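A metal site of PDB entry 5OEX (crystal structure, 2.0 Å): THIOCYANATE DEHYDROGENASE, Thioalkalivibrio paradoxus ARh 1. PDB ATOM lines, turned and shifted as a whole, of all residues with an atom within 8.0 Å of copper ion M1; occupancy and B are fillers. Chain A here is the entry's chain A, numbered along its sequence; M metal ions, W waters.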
ATOM      1  N   HIS A  54      11.500 -36.991  -4.131  1.00  0.00           N
ATOM      2  CA  HIS A  54      12.197 -35.702  -4.321  1.00  0.00           C
ATOM      3  C   HIS A  54      12.211 -34.750  -3.095  1.00  0.00           C
ATOM      4  O   HIS A  54      13.114 -34.823  -2.258  1.00  0.00           O
ATOM      5  CB  HIS A  54      11.807 -34.978  -5.621  1.00  0.00           C
ATOM      6  CG  HIS A  54      12.792 -33.914  -5.979  1.00  0.00           C
ATOM      7  ND1 HIS A  54      12.480 -32.824  -6.757  1.00  0.00           N
ATOM      8  CD2 HIS A  54      14.099 -33.787  -5.634  1.00  0.00           C
ATOM      9  CE1 HIS A  54      13.558 -32.066  -6.905  1.00  0.00           C
ATOM     10  NE2 HIS A  54      14.536 -32.609  -6.177  1.00  0.00           N
ATOM     11  N   HIS A  55      11.195 -33.910  -2.916  1.00  0.00           N
ATOM     12  CA  HIS A  55      11.233 -33.067  -1.780  1.00  0.00           C
ATOM     13  C   HIS A  55      10.179 -33.514  -0.822  1.00  0.00           C
ATOM     14  O   HIS A  55       9.335 -34.306  -1.233  1.00  0.00           O
ATOM     15  CB  HIS A  55      11.003 -31.646  -2.188  1.00  0.00           C
ATOM     16  CG  HIS A  55      12.211 -31.077  -2.841  1.00  0.00           C
ATOM     17  ND1 HIS A  55      13.368 -30.862  -2.138  1.00  0.00           N
ATOM     18  CD2 HIS A  55      12.467 -30.751  -4.137  1.00  0.00           C
ATOM     19  CE1 HIS A  55      14.293 -30.379  -2.949  1.00  0.00           C
ATOM     20  NE2 HIS A  55      13.775 -30.303  -4.156  1.00  0.00           N
ATOM     21  N   VAL A 124       8.937 -30.225  -7.577  1.00  0.00           N
ATOM     22  CA  VAL A 124      10.066 -29.548  -6.903  1.00  0.00           C
ATOM     23  C   VAL A 124       9.699 -29.356  -5.430  1.00  0.00           C
ATOM     24  O   VAL A 124       9.259 -30.350  -4.811  1.00  0.00           O
ATOM     25  CB  VAL A 124      10.655 -28.363  -7.722  1.00  0.00           C
ATOM     26  CG1 VAL A 124      12.080 -28.010  -7.240  1.00  0.00           C
ATOM     27  CG2 VAL A 124      10.751 -28.803  -9.214  1.00  0.00           C
ATOM     28  N   HIS A 125       9.898 -28.185  -4.842  1.00  0.00           N
ATOM     29  CA  HIS A 125       9.883 -28.100  -3.339  1.00  0.00           C
ATOM     30  C   HIS A 125       8.509 -28.229  -2.759  1.00  0.00           C
ATOM     31  O   HIS A 125       7.544 -27.712  -3.348  1.00  0.00           O
ATOM     32  CB  HIS A 125      10.481 -26.751  -2.854  1.00  0.00           C
ATOM     33  CG  HIS A 125      11.974 -26.679  -3.000  1.00  0.00           C
ATOM     34  ND1 HIS A 125      12.827 -27.309  -2.145  1.00  0.00           N
ATOM     35  CD2 HIS A 125      12.760 -26.097  -3.949  1.00  0.00           C
ATOM     36  CE1 HIS A 125      14.073 -27.114  -2.526  1.00  0.00           C
ATOM     37  NE2 HIS A 125      14.063 -26.392  -3.614  1.00  0.00           N
ATOM     38  N   GLU A 207      14.101 -30.838 -14.662  1.00  0.00           N
ATOM     39  CA  GLU A 207      14.337 -29.678 -13.798  1.00  0.00           C
ATOM     40  C   GLU A 207      15.760 -29.165 -14.109  1.00  0.00           C
ATOM     41  O   GLU A 207      16.661 -30.005 -14.266  1.00  0.00           O
ATOM     42  CB  GLU A 207      14.329 -30.122 -12.324  1.00  0.00           C
ATOM     43  CG  GLU A 207      14.452 -28.944 -11.322  1.00  0.00           C
ATOM     44  CD  GLU A 207      14.717 -29.397  -9.850  1.00  0.00           C
ATOM     45  OE1 GLU A 207      14.816 -30.605  -9.575  1.00  0.00           O
ATOM     46  OE2 GLU A 207      14.910 -28.526  -8.967  1.00  0.00           O
ATOM     47  N   ASN A 232      10.238 -21.832 -11.790  1.00  0.00           N
ATOM     48  CA  ASN A 232       9.754 -21.767 -10.416  1.00  0.00           C
ATOM     49  C   ASN A 232      10.412 -22.908  -9.602  1.00  0.00           C
ATOM     50  O   ASN A 232      10.688 -23.999 -10.133  1.00  0.00           O
ATOM     51  CB  ASN A 232       8.228 -21.892 -10.404  1.00  0.00           C
ATOM     52  CG  ASN A 232       7.652 -21.946  -8.986  1.00  0.00           C
ATOM     53  OD1 ASN A 232       7.033 -22.947  -8.587  1.00  0.00           O
ATOM     54  ND2 ASN A 232       7.895 -20.911  -8.193  1.00  0.00           N
ATOM     55  N   ASP A 233      10.698 -22.651  -8.337  1.00  0.00           N
ATOM     56  CA  ASP A 233      11.452 -23.654  -7.516  1.00  0.00           C
ATOM     57  C   ASP A 233      10.602 -24.003  -6.299  1.00  0.00           C
ATOM     58  O   ASP A 233      10.318 -25.178  -6.055  1.00  0.00           O
ATOM     59  CB  ASP A 233      12.868 -23.067  -7.229  1.00  0.00           C
ATOM     60  CG  ASP A 233      13.690 -23.862  -6.164  1.00  0.00           C
ATOM     61  OD1 ASP A 233      13.814 -23.282  -5.035  1.00  0.00           O
ATOM     62  OD2 ASP A 233      14.302 -24.951  -6.432  1.00  0.00           O
ATOM     63  N   ALA A 234      10.059 -22.973  -5.647  1.00  0.00           N
ATOM     64  CA  ALA A 234       9.358 -23.122  -4.366  1.00  0.00           C
ATOM     65  C   ALA A 234       8.252 -22.089  -4.089  1.00  0.00           C
ATOM     66  O   ALA A 234       8.241 -20.980  -4.652  1.00  0.00           O
ATOM     67  CB  ALA A 234      10.364 -23.120  -3.202  1.00  0.00           C
ATOM     68  N   SER A 247       9.562 -18.438  -5.783  1.00  0.00           N
ATOM     69  CA  SER A 247      10.868 -18.071  -6.358  1.00  0.00           C
ATOM     70  C   SER A 247      10.983 -18.508  -7.821  1.00  0.00           C
ATOM     71  O   SER A 247      10.526 -19.601  -8.186  1.00  0.00           O
ATOM     72  CB  SER A 247      12.001 -18.689  -5.546  1.00  0.00           C
ATOM     73  OG  SER A 247      11.729 -20.081  -5.389  1.00  0.00           O
ATOM     74  N   ARG A 249      13.773 -19.064 -10.662  1.00  0.00           N
ATOM     75  CA  ARG A 249      15.205 -19.173 -10.876  1.00  0.00           C
ATOM     76  C   ARG A 249      15.698 -18.345 -12.075  1.00  0.00           C
ATOM     77  O   ARG A 249      16.545 -17.506 -11.881  1.00  0.00           O
ATOM     78  CB  ARG A 249      15.638 -20.604 -10.925  1.00  0.00           C
ATOM     79  CG  ARG A 249      15.406 -21.378  -9.599  1.00  0.00           C
ATOM     80  CD  ARG A 249      15.692 -22.863  -9.810  1.00  0.00           C
ATOM     81  NE  ARG A 249      17.041 -23.049 -10.360  1.00  0.00           N
ATOM     82  CZ  ARG A 249      17.530 -24.196 -10.833  1.00  0.00           C
ATOM     83  NH1 ARG A 249      16.783 -25.294 -10.828  1.00  0.00           N
ATOM     84  NH2 ARG A 249      18.761 -24.265 -11.334  1.00  0.00           N
ATOM     85  N   GLY A 299      18.693 -16.869  -9.684  1.00  0.00           N
ATOM     86  CA  GLY A 299      18.682 -17.046  -8.224  1.00  0.00           C
ATOM     87  C   GLY A 299      18.119 -18.423  -7.816  1.00  0.00           C
ATOM     88  O   GLY A 299      17.594 -19.161  -8.626  1.00  0.00           O
ATOM     89  N   HIS A 300      18.202 -18.801  -6.562  1.00  0.00           N
ATOM     90  CA  HIS A 300      17.611 -20.081  -6.172  1.00  0.00           C
ATOM     91  C   HIS A 300      16.950 -20.050  -4.816  1.00  0.00           C
ATOM     92  O   HIS A 300      15.769 -19.787  -4.735  1.00  0.00           O
ATOM     93  CB  HIS A 300      18.630 -21.232  -6.214  1.00  0.00           C
ATOM     94  CG  HIS A 300      18.011 -22.597  -6.203  1.00  0.00           C
ATOM     95  ND1 HIS A 300      18.429 -23.604  -7.059  1.00  0.00           N
ATOM     96  CD2 HIS A 300      17.021 -23.137  -5.440  1.00  0.00           C
ATOM     97  CE1 HIS A 300      17.717 -24.702  -6.827  1.00  0.00           C
ATOM     98  NE2 HIS A 300      16.846 -24.443  -5.879  1.00  0.00           N
ATOM     99  N   GLN A 301      17.710 -20.336  -3.761  1.00  0.00           N
ATOM    100  CA  GLN A 301      17.149 -20.437  -2.419  1.00  0.00           C
ATOM    101  C   GLN A 301      16.414 -19.189  -1.970  1.00  0.00           C
ATOM    102  O   GLN A 301      16.888 -18.062  -2.219  1.00  0.00           O
ATOM    103  CB  GLN A 301      18.302 -20.777  -1.456  1.00  0.00           C
ATOM    104  CG  GLN A 301      18.033 -20.642   0.060  1.00  0.00           C
ATOM    105  CD  GLN A 301      16.816 -21.452   0.524  1.00  0.00           C
ATOM    106  OE1 GLN A 301      16.572 -22.548   0.008  1.00  0.00           O
ATOM    107  NE2 GLN A 301      16.039 -20.906   1.466  1.00  0.00           N
ATOM    108  N   ALA A 302      15.275 -19.348  -1.294  1.00  0.00           N
ATOM    109  CA  ALA A 302      14.463 -18.197  -0.841  1.00  0.00           C
ATOM    110  C   ALA A 302      13.830 -18.482   0.510  1.00  0.00           C
ATOM    111  O   ALA A 302      13.319 -19.550   0.730  1.00  0.00           O
ATOM    112  CB  ALA A 302      13.378 -17.943  -1.849  1.00  0.00           C
ATOM    113  N   PHE A 355      22.151 -23.477  -1.963  1.00  0.00           N
ATOM    114  CA  PHE A 355      20.702 -23.686  -2.344  1.00  0.00           C
ATOM    115  C   PHE A 355      19.786 -23.982  -1.172  1.00  0.00           C
ATOM    116  O   PHE A 355      18.538 -24.184  -1.354  1.00  0.00           O
ATOM    117  CB  PHE A 355      20.489 -24.838  -3.350  1.00  0.00           C
ATOM    118  CG  PHE A 355      21.271 -24.718  -4.612  1.00  0.00           C
ATOM    119  CD1 PHE A 355      21.236 -23.541  -5.388  1.00  0.00           C
ATOM    120  CD2 PHE A 355      22.013 -25.807  -5.079  1.00  0.00           C
ATOM    121  CE1 PHE A 355      21.966 -23.429  -6.580  1.00  0.00           C
ATOM    122  CE2 PHE A 355      22.732 -25.692  -6.264  1.00  0.00           C
ATOM    123  CZ  PHE A 355      22.693 -24.503  -7.025  1.00  0.00           C
ATOM    124  N   HIS A 356      20.391 -24.104   0.001  1.00  0.00           N
ATOM    125  CA  HIS A 356      19.628 -24.536   1.187  1.00  0.00           C
ATOM    126  C   HIS A 356      20.090 -23.767   2.435  1.00  0.00           C
ATOM    127  O   HIS A 356      21.290 -23.428   2.589  1.00  0.00           O
ATOM    128  CB  HIS A 356      19.698 -26.067   1.370  1.00  0.00           C
ATOM    129  CG  HIS A 356      19.319 -26.874   0.147  1.00  0.00           C
ATOM    130  ND1 HIS A 356      18.018 -27.014  -0.263  1.00  0.00           N
ATOM    131  CD2 HIS A 356      20.053 -27.601  -0.744  1.00  0.00           C
ATOM    132  CE1 HIS A 356      17.949 -27.791  -1.343  1.00  0.00           C
ATOM    133  NE2 HIS A 356      19.167 -28.197  -1.638  1.00  0.00           N
ATOM    134  N   THR A 402      20.263 -30.613   1.790  1.00  0.00           N
ATOM    135  CA  THR A 402      19.510 -29.826   2.758  1.00  0.00           C
ATOM    136  C   THR A 402      20.057 -29.844   4.184  1.00  0.00           C
ATOM    137  O   THR A 402      20.907 -30.663   4.528  1.00  0.00           O
ATOM    138  CB  THR A 402      18.030 -30.218   2.755  1.00  0.00           C
ATOM    139  OG1 THR A 402      17.986 -31.660   2.764  1.00  0.00           O
ATOM    140  CG2 THR A 402      17.358 -29.604   1.508  1.00  0.00           C
ATOM    141  N   HIS A 447      17.584 -35.231  -1.624  1.00  0.00           N
ATOM    142  CA  HIS A 447      17.582 -33.823  -1.849  1.00  0.00           C
ATOM    143  C   HIS A 447      16.710 -33.061  -0.840  1.00  0.00           C
ATOM    144  O   HIS A 447      16.334 -31.873  -1.053  1.00  0.00           O
ATOM    145  CB  HIS A 447      17.112 -33.530  -3.289  1.00  0.00           C
ATOM    146  CG  HIS A 447      18.158 -33.810  -4.317  1.00  0.00           C
ATOM    147  ND1 HIS A 447      18.124 -33.241  -5.564  1.00  0.00           N
ATOM    148  CD2 HIS A 447      19.284 -34.582  -4.289  1.00  0.00           C
ATOM    149  CE1 HIS A 447      19.141 -33.703  -6.292  1.00  0.00           C
ATOM    150  NE2 HIS A 447      19.892 -34.472  -5.524  1.00  0.00           N
ATOM    151  N   THR A 467      13.754 -23.419   2.140  1.00  0.00           N
ATOM    152  CA  THR A 467      14.085 -24.732   1.550  1.00  0.00           C
ATOM    153  C   THR A 467      15.580 -25.170   1.734  1.00  0.00           C
ATOM    154  O   THR A 467      15.945 -26.282   1.229  1.00  0.00           O
ATOM    155  CB  THR A 467      13.637 -24.834   0.061  1.00  0.00           C
ATOM    156  OG1 THR A 467      14.365 -23.953  -0.785  1.00  0.00           O
ATOM    157  CG2 THR A 467      12.124 -24.555  -0.069  1.00  0.00           C
ATOM    158  OXT THR A 467      16.424 -24.479   2.403  1.00  0.00           O
HETATM  159 CU    CU M   1      15.449 -25.448  -4.782  1.00  0.00          CU
HETATM  160 CU    CU M   2      18.976 -30.205  -2.480  1.00  0.00          CU
HETATM  161 CU    CU M   3      16.537 -31.846  -5.943  1.00  0.00          CU
HETATM  162 CU    CU M   4      16.484 -32.796  -6.551  1.00  0.00          CU
HETATM  163  O   HOH W   1      16.203 -24.964  -2.868  1.00  0.00           O
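The backbone NH (N) of Asp 233 is in hydrogen-bond range of the backbone carbonyl oxygen (O) of Ser 247 (3.1 Å).
Of the 19 residues printed, 3 come within 4 Å of copper ion M1. The nearest printed residue that does not touch copper ion M1 is Thr 467 (4.4 Å).
A ring nitrogen (NE2) of His 300 binds copper ion M1, at 2.0 Å. Copper ion M1 is bound by NE2 of His 125 (2.0 Å). OD2 of Asp 233 is bound to copper ion M1 (2.1 Å). Copper ion M1 is bound by water W1, at 2.1 Å. Copper ion M1 has four donor atoms within binding distance. Slightly farther from copper ion M1 lies the side-chain carboxylate (OD1) of Asp 233 (2.7 Å).
Water W1 lies within hydrogen-bond range of the backbone carbonyl oxygen (O) of Phe 355 (2.9 Å) and the side-chain hydroxyl (OG1) of Thr 467 (3.0 Å).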
